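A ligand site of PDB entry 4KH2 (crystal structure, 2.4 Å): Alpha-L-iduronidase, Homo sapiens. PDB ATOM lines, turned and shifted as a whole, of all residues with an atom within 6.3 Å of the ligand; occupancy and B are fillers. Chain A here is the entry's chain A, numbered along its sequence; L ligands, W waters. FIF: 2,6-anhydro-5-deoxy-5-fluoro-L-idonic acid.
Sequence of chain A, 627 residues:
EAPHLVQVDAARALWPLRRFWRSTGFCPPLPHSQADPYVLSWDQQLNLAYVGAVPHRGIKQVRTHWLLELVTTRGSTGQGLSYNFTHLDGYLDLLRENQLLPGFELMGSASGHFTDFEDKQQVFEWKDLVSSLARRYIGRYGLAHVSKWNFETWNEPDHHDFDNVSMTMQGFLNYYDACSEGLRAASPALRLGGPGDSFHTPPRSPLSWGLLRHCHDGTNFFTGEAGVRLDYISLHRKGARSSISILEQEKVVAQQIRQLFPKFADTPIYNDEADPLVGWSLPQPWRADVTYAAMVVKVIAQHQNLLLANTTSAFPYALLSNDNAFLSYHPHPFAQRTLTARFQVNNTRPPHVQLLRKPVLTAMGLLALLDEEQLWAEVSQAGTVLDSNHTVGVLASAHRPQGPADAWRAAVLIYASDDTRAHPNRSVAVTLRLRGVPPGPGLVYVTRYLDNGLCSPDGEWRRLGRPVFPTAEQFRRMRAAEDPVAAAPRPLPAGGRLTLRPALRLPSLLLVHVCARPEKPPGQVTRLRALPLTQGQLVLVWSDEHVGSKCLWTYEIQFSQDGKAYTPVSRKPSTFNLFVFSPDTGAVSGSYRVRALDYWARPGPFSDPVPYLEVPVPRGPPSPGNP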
ATOM      1  N   PHE A  26      -2.405 -16.388 -24.551  1.00  0.00           N
ATOM      2  CA  PHE A  26      -2.538 -16.314 -23.091  1.00  0.00           C
ATOM      3  C   PHE A  26      -3.968 -15.996 -22.663  1.00  0.00           C
ATOM      4  O   PHE A  26      -4.836 -15.676 -23.492  1.00  0.00           O
ATOM      5  CB  PHE A  26      -1.579 -15.280 -22.493  1.00  0.00           C
ATOM      6  CG  PHE A  26      -2.016 -13.855 -22.674  1.00  0.00           C
ATOM      7  CD1 PHE A  26      -1.666 -13.161 -23.824  1.00  0.00           C
ATOM      8  CD2 PHE A  26      -2.753 -13.204 -21.700  1.00  0.00           C
ATOM      9  CE1 PHE A  26      -2.068 -11.843 -24.002  1.00  0.00           C
ATOM     10  CE2 PHE A  26      -3.158 -11.889 -21.865  1.00  0.00           C
ATOM     11  CZ  PHE A  26      -2.805 -11.205 -23.016  1.00  0.00           C
ATOM     12  N   CYS A  27      -4.193 -16.062 -21.356  1.00  0.00           N
ATOM     13  CA  CYS A  27      -5.476 -15.743 -20.736  1.00  0.00           C
ATOM     14  C   CYS A  27      -5.259 -14.777 -19.561  1.00  0.00           C
ATOM     15  O   CYS A  27      -4.361 -14.989 -18.750  1.00  0.00           O
ATOM     16  CB  CYS A  27      -6.136 -17.036 -20.236  1.00  0.00           C
ATOM     17  SG  CYS A  27      -7.761 -16.823 -19.499  1.00  0.00           S
ATOM     18  N   ARG A  63      -3.039 -15.341 -29.473  1.00  0.00           N
ATOM     19  CA  ARG A  63      -4.396 -15.817 -29.233  1.00  0.00           C
ATOM     20  C   ARG A  63      -4.838 -15.471 -27.816  1.00  0.00           C
ATOM     21  O   ARG A  63      -4.471 -16.151 -26.859  1.00  0.00           O
ATOM     22  CB  ARG A  63      -4.482 -17.329 -29.489  1.00  0.00           C
ATOM     23  CG  ARG A  63      -5.889 -17.883 -29.624  1.00  0.00           C
ATOM     24  CD  ARG A  63      -5.874 -19.400 -29.730  1.00  0.00           C
ATOM     25  NE  ARG A  63      -7.215 -19.976 -29.684  1.00  0.00           N
ATOM     26  CZ  ARG A  63      -7.759 -20.555 -28.619  1.00  0.00           C
ATOM     27  NH1 ARG A  63      -7.087 -20.642 -27.471  1.00  0.00           N
ATOM     28  NH2 ARG A  63      -8.985 -21.065 -28.685  1.00  0.00           N
ATOM     29  N   HIS A  65      -7.559 -14.622 -24.780  1.00  0.00           N
ATOM     30  CA  HIS A  65      -8.884 -14.851 -24.202  1.00  0.00           C
ATOM     31  C   HIS A  65      -9.575 -13.563 -23.753  1.00  0.00           C
ATOM     32  O   HIS A  65      -8.923 -12.538 -23.589  1.00  0.00           O
ATOM     33  CB  HIS A  65      -8.795 -15.751 -22.969  1.00  0.00           C
ATOM     34  CG  HIS A  65      -8.566 -17.196 -23.290  1.00  0.00           C
ATOM     35  ND1 HIS A  65      -7.648 -17.627 -24.220  1.00  0.00           N
ATOM     36  CD2 HIS A  65      -9.104 -18.309 -22.746  1.00  0.00           C
ATOM     37  CE1 HIS A  65      -7.651 -18.949 -24.259  1.00  0.00           C
ATOM     38  NE2 HIS A  65      -8.528 -19.389 -23.373  1.00  0.00           N
ATOM     39  N   GLU A 105     -10.482 -14.276 -30.391  1.00  0.00           N
ATOM     40  CA  GLU A 105     -11.567 -15.106 -29.891  1.00  0.00           C
ATOM     41  C   GLU A 105     -12.751 -14.223 -29.525  1.00  0.00           C
ATOM     42  O   GLU A 105     -12.622 -13.278 -28.750  1.00  0.00           O
ATOM     43  CB  GLU A 105     -11.123 -15.913 -28.678  1.00  0.00           C
ATOM     44  CG  GLU A 105      -9.928 -16.819 -28.957  1.00  0.00           C
ATOM     45  CD  GLU A 105      -9.321 -17.350 -27.689  1.00  0.00           C
ATOM     46  OE1 GLU A 105      -8.179 -16.934 -27.366  1.00  0.00           O
ATOM     47  OE2 GLU A 105      -9.981 -18.154 -27.006  1.00  0.00           O
ATOM     48  N   ASN A 155     -13.460 -19.731 -26.453  1.00  0.00           N
ATOM     49  CA  ASN A 155     -12.533 -20.825 -26.140  1.00  0.00           C
ATOM     50  C   ASN A 155     -13.205 -22.021 -25.483  1.00  0.00           C
ATOM     51  O   ASN A 155     -14.131 -21.857 -24.675  1.00  0.00           O
ATOM     52  CB  ASN A 155     -11.368 -20.348 -25.266  1.00  0.00           C
ATOM     53  CG  ASN A 155     -10.243 -21.382 -25.182  1.00  0.00           C
ATOM     54  OD1 ASN A 155      -9.600 -21.695 -26.184  1.00  0.00           O
ATOM     55  ND2 ASN A 155     -10.018 -21.915 -23.982  1.00  0.00           N
ATOM     56  N   GLU A 156     -12.735 -23.213 -25.841  1.00  0.00           N
ATOM     57  CA  GLU A 156     -13.200 -24.477 -25.280  1.00  0.00           C
ATOM     58  C   GLU A 156     -14.667 -24.470 -24.841  1.00  0.00           C
ATOM     59  O   GLU A 156     -14.949 -24.514 -23.640  1.00  0.00           O
ATOM     60  CB  GLU A 156     -12.280 -24.912 -24.123  1.00  0.00           C
ATOM     61  CG  GLU A 156     -10.855 -25.230 -24.560  1.00  0.00           C
ATOM     62  CD  GLU A 156      -9.911 -25.520 -23.406  1.00  0.00           C
ATOM     63  OE1 GLU A 156     -10.336 -25.487 -22.227  1.00  0.00           O
ATOM     64  OE2 GLU A 156      -8.730 -25.793 -23.680  1.00  0.00           O
ATOM     65  N   HIS A 236      -7.821 -28.466 -29.657  1.00  0.00           N
ATOM     66  CA  HIS A 236      -6.803 -28.396 -28.605  1.00  0.00           C
ATOM     67  C   HIS A 236      -6.334 -29.799 -28.246  1.00  0.00           C
ATOM     68  O   HIS A 236      -7.102 -30.586 -27.675  1.00  0.00           O
ATOM     69  CB  HIS A 236      -7.336 -27.721 -27.345  1.00  0.00           C
ATOM     70  CG  HIS A 236      -7.730 -26.282 -27.528  1.00  0.00           C
ATOM     71  ND1 HIS A 236      -7.385 -25.536 -28.628  1.00  0.00           N
ATOM     72  CD2 HIS A 236      -8.426 -25.453 -26.716  1.00  0.00           C
ATOM     73  CE1 HIS A 236      -7.863 -24.316 -28.497  1.00  0.00           C
ATOM     74  NE2 HIS A 236      -8.492 -24.238 -27.341  1.00  0.00           N
ATOM     75  N   LYS A 238      -2.985 -31.733 -26.333  1.00  0.00           N
ATOM     76  CA  LYS A 238      -1.737 -31.659 -25.563  1.00  0.00           C
ATOM     77  C   LYS A 238      -1.141 -33.056 -25.381  1.00  0.00           C
ATOM     78  O   LYS A 238      -1.854 -34.054 -25.440  1.00  0.00           O
ATOM     79  CB  LYS A 238      -1.996 -30.967 -24.217  1.00  0.00           C
ATOM     80  CG  LYS A 238      -2.384 -29.500 -24.370  1.00  0.00           C
ATOM     81  CD  LYS A 238      -3.571 -29.156 -23.481  1.00  0.00           C
ATOM     82  CE  LYS A 238      -3.904 -27.673 -23.504  1.00  0.00           C
ATOM     83  NZ  LYS A 238      -2.813 -26.742 -23.050  1.00  0.00           N
ATOM     84  N   GLU A 273      -3.671 -24.795 -29.140  1.00  0.00           N
ATOM     85  CA  GLU A 273      -2.895 -25.004 -27.901  1.00  0.00           C
ATOM     86  C   GLU A 273      -2.308 -26.408 -27.933  1.00  0.00           C
ATOM     87  O   GLU A 273      -2.883 -27.395 -27.448  1.00  0.00           O
ATOM     88  CB  GLU A 273      -3.633 -24.593 -26.590  1.00  0.00           C
ATOM     89  CG  GLU A 273      -5.010 -25.114 -26.374  1.00  0.00           C
ATOM     90  CD  GLU A 273      -5.483 -25.136 -24.914  1.00  0.00           C
ATOM     91  OE1 GLU A 273      -6.194 -26.062 -24.536  1.00  0.00           O
ATOM     92  OE2 GLU A 273      -5.133 -24.111 -23.954  1.00  0.00           O
ATOM     93  N   ASP A 275       0.475 -27.740 -26.527  1.00  0.00           N
ATOM     94  CA  ASP A 275       1.503 -27.685 -25.492  1.00  0.00           C
ATOM     95  C   ASP A 275       1.880 -29.079 -24.988  1.00  0.00           C
ATOM     96  O   ASP A 275       1.016 -29.974 -24.937  1.00  0.00           O
ATOM     97  CB  ASP A 275       1.053 -26.796 -24.338  1.00  0.00           C
ATOM     98  CG  ASP A 275       0.672 -25.399 -24.805  1.00  0.00           C
ATOM     99  OD1 ASP A 275       1.560 -24.640 -25.250  1.00  0.00           O
ATOM    100  OD2 ASP A 275      -0.530 -25.068 -24.716  1.00  0.00           O
ATOM    101  N   LEU A 277       2.273 -30.126 -22.014  1.00  0.00           N
ATOM    102  CA  LEU A 277       1.529 -30.493 -20.824  1.00  0.00           C
ATOM    103  C   LEU A 277       0.488 -29.439 -20.449  1.00  0.00           C
ATOM    104  O   LEU A 277       0.815 -28.259 -20.354  1.00  0.00           O
ATOM    105  CB  LEU A 277       2.490 -30.728 -19.645  1.00  0.00           C
ATOM    106  CG  LEU A 277       1.926 -30.960 -18.237  1.00  0.00           C
ATOM    107  CD1 LEU A 277       1.235 -32.314 -18.110  1.00  0.00           C
ATOM    108  CD2 LEU A 277       3.016 -30.803 -17.191  1.00  0.00           C
ATOM    109  N   VAL A 278      -0.740 -29.894 -20.226  1.00  0.00           N
ATOM    110  CA  VAL A 278      -1.837 -29.028 -19.784  1.00  0.00           C
ATOM    111  C   VAL A 278      -1.533 -28.406 -18.428  1.00  0.00           C
ATOM    112  O   VAL A 278      -0.886 -29.032 -17.585  1.00  0.00           O
ATOM    113  CB  VAL A 278      -3.186 -29.816 -19.755  1.00  0.00           C
ATOM    114  CG1 VAL A 278      -3.180 -30.897 -18.670  1.00  0.00           C
ATOM    115  CG2 VAL A 278      -4.364 -28.868 -19.567  1.00  0.00           C
ATOM    116  N   GLY A 279      -1.976 -27.168 -18.224  1.00  0.00           N
ATOM    117  CA  GLY A 279      -1.794 -26.453 -16.948  1.00  0.00           C
ATOM    118  C   GLY A 279      -0.539 -25.598 -16.923  1.00  0.00           C
ATOM    119  O   GLY A 279       0.496 -26.004 -16.397  1.00  0.00           O
ATOM    120  N   TRP A 280      -0.656 -24.391 -17.472  1.00  0.00           N
ATOM    121  CA  TRP A 280       0.481 -23.470 -17.668  1.00  0.00           C
ATOM    122  C   TRP A 280       1.189 -23.061 -16.381  1.00  0.00           C
ATOM    123  O   TRP A 280       2.401 -22.830 -16.387  1.00  0.00           O
ATOM    124  CB  TRP A 280       0.011 -22.222 -18.418  1.00  0.00           C
ATOM    125  CG  TRP A 280      -0.687 -21.203 -17.537  1.00  0.00           C
ATOM    126  CD1 TRP A 280      -2.035 -21.129 -17.270  1.00  0.00           C
ATOM    127  CD2 TRP A 280      -0.074 -20.142 -16.797  1.00  0.00           C
ATOM    128  NE1 TRP A 280      -2.283 -20.081 -16.417  1.00  0.00           N
ATOM    129  CE2 TRP A 280      -1.100 -19.458 -16.107  1.00  0.00           C
ATOM    130  CE3 TRP A 280       1.251 -19.701 -16.650  1.00  0.00           C
ATOM    131  CZ2 TRP A 280      -0.850 -18.355 -15.287  1.00  0.00           C
ATOM    132  CZ3 TRP A 280       1.504 -18.608 -15.831  1.00  0.00           C
ATOM    133  CH2 TRP A 280       0.453 -17.949 -15.160  1.00  0.00           C
ATOM    134  N   SER A 281       0.436 -22.956 -15.292  1.00  0.00           N
ATOM    135  CA  SER A 281       0.933 -22.360 -14.046  1.00  0.00           C
ATOM    136  C   SER A 281       1.644 -23.377 -13.158  1.00  0.00           C
ATOM    137  O   SER A 281       2.393 -22.992 -12.264  1.00  0.00           O
ATOM    138  CB  SER A 281      -0.214 -21.698 -13.262  1.00  0.00           C
ATOM    139  OG  SER A 281      -1.204 -22.652 -12.920  1.00  0.00           O
ATOM    140  N   ASP A 323       0.806 -22.166 -26.464  1.00  0.00           N
ATOM    141  CA  ASP A 323       0.030 -21.208 -25.676  1.00  0.00           C
ATOM    142  C   ASP A 323       0.831 -20.758 -24.454  1.00  0.00           C
ATOM    143  O   ASP A 323       0.520 -21.150 -23.317  1.00  0.00           O
ATOM    144  CB  ASP A 323      -1.277 -21.863 -25.245  1.00  0.00           C
ATOM    145  CG  ASP A 323      -2.306 -20.866 -24.762  1.00  0.00           C
ATOM    146  OD1 ASP A 323      -2.320 -19.724 -25.243  1.00  0.00           O
ATOM    147  OD2 ASP A 323      -3.139 -21.242 -23.924  1.00  0.00           O
ATOM    148  N   PHE A 326       1.830 -16.154 -21.311  1.00  0.00           N
ATOM    149  CA  PHE A 326       1.491 -15.798 -19.941  1.00  0.00           C
ATOM    150  C   PHE A 326       2.657 -15.096 -19.265  1.00  0.00           C
ATOM    151  O   PHE A 326       3.823 -15.302 -19.646  1.00  0.00           O
ATOM    152  CB  PHE A 326       1.159 -17.055 -19.122  1.00  0.00           C
ATOM    153  CG  PHE A 326      -0.075 -17.786 -19.575  1.00  0.00           C
ATOM    154  CD1 PHE A 326      -1.321 -17.472 -19.045  1.00  0.00           C
ATOM    155  CD2 PHE A 326       0.018 -18.814 -20.512  1.00  0.00           C
ATOM    156  CE1 PHE A 326      -2.454 -18.147 -19.452  1.00  0.00           C
ATOM    157  CE2 PHE A 326      -1.111 -19.499 -20.922  1.00  0.00           C
ATOM    158  CZ  PHE A 326      -2.356 -19.162 -20.392  1.00  0.00           C
ATOM    159  N   ARG A 337       4.846 -22.209 -17.933  1.00  0.00           N
ATOM    160  CA  ARG A 337       4.832 -22.251 -19.412  1.00  0.00           C
ATOM    161  C   ARG A 337       4.723 -20.835 -19.990  1.00  0.00           C
ATOM    162  O   ARG A 337       3.648 -20.408 -20.400  1.00  0.00           O
ATOM    163  CB  ARG A 337       3.701 -23.150 -19.935  1.00  0.00           C
ATOM    164  CG  ARG A 337       3.866 -23.588 -21.389  1.00  0.00           C
ATOM    165  CD  ARG A 337       2.535 -23.749 -22.111  1.00  0.00           C
ATOM    166  NE  ARG A 337       1.703 -24.802 -21.525  1.00  0.00           N
ATOM    167  CZ  ARG A 337       0.388 -24.690 -21.300  1.00  0.00           C
ATOM    168  NH1 ARG A 337      -0.272 -25.701 -20.767  1.00  0.00           N
ATOM    169  NH2 ARG A 337      -0.251 -23.572 -21.606  1.00  0.00           N
HETATM  170  O6B FIF L   1      -3.671 -23.984 -18.625  1.00  0.00           O
HETATM  171  C6  FIF L   1      -3.816 -24.420 -19.785  1.00  0.00           C
HETATM  172  O6A FIF L   1      -3.086 -25.306 -20.281  1.00  0.00           O
HETATM  173  C5  FIF L   1      -4.911 -23.817 -20.635  1.00  0.00           C
HETATM  174  O5  FIF L   1      -5.313 -24.702 -21.692  1.00  0.00           O
HETATM  175  C4  FIF L   1      -4.374 -22.498 -21.203  1.00  0.00           C
HETATM  176  O4  FIF L   1      -3.200 -22.758 -21.991  1.00  0.00           O
HETATM  177  C3  FIF L   1      -5.434 -21.767 -22.050  1.00  0.00           C
HETATM  178  O3  FIF L   1      -5.989 -20.693 -21.285  1.00  0.00           O
HETATM  179  C2  FIF L   1      -6.542 -22.720 -22.528  1.00  0.00           C
HETATM  180  F2  FIF L   1      -7.152 -22.205 -23.644  1.00  0.00           F
HETATM  181  C1  FIF L   1      -6.002 -24.123 -22.832  1.00  0.00           C
HETATM  182  O   HOH W   1      -7.902 -26.354 -20.220  1.00  0.00           O
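NE2 of His 65 lies close to F2 of the ligand, 3.1 Å away. ND2 of Asn 155 lies close to F2 of the ligand, 2.9 Å away. CB of Cys 27 touches O3 of the ligand, 3.8 Å away. Glu 156 touches the ligand. Val 278 touches the ligand. Phe 326 touches the ligand (CZ to C4, 3.98 Å). Hydrophobic or aromatic side chains within 4 Å of the ligand: His 65, Val 278, Trp 280 and Phe 326. Within 4 Å of the ligand: Cys 27, His 65, Asn 155, Glu 156, Lys 238, Glu 273, Val 278, Gly 279, Trp 280, Asp 323, Phe 326 and Arg 337.
The side-chain carboxylate (OE2) of Glu 273 is bonded to a carbon (C1) of the ligand, 1.4 Å away. O6A of the ligand is in hydrogen-bond range of N of Gly 279 (3.0 Å). N of Trp 280 lies within hydrogen-bond range of O6B of the ligand, 3.3 Å away. NH1 of Arg 337 is in salt-bridge range of O6A of the ligand, 2.9 Å away. An oxygen (O4) of the ligand lies within hydrogen-bond range of the side-chain carboxylate of Asp 323 (2.5 Å). NZ of Lys 238 lies within salt-bridge range of O6A of the ligand (3.1 Å).
N of Phe 26 sits at hydrogen-bond distance from OD1 of Asp 323 (3.4 Å). O of Phe 26 lies within hydrogen-bond range of N of His 65. The side-chain amide nitrogen of Asn 155 lies within hydrogen-bond range of a ring nitrogen (NE2) of His 65, at 3.0 Å. OD2 of Asp 275 lies within salt-bridge range of NZ of Lys 238, at 3.3 Å. The side-chain amide oxygen (OD1) of Asn 155 lies within hydrogen-bond range of a ring nitrogen (NE2) of His 236 (3.0 Å). OE2 of Glu 273 is in salt-bridge range of NZ of Lys 238 (3.6 Å). O of Trp 280 lies within hydrogen-bond range of N of Arg 337. The side-chain carboxylate of Asp 275 lies within salt-bridge range of the guanidinium group of Arg 337 (3.5 Å).
Water W1 bridges OE1 of Glu 156 (3.3 Å) and O5 of the ligand (3.4 Å).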
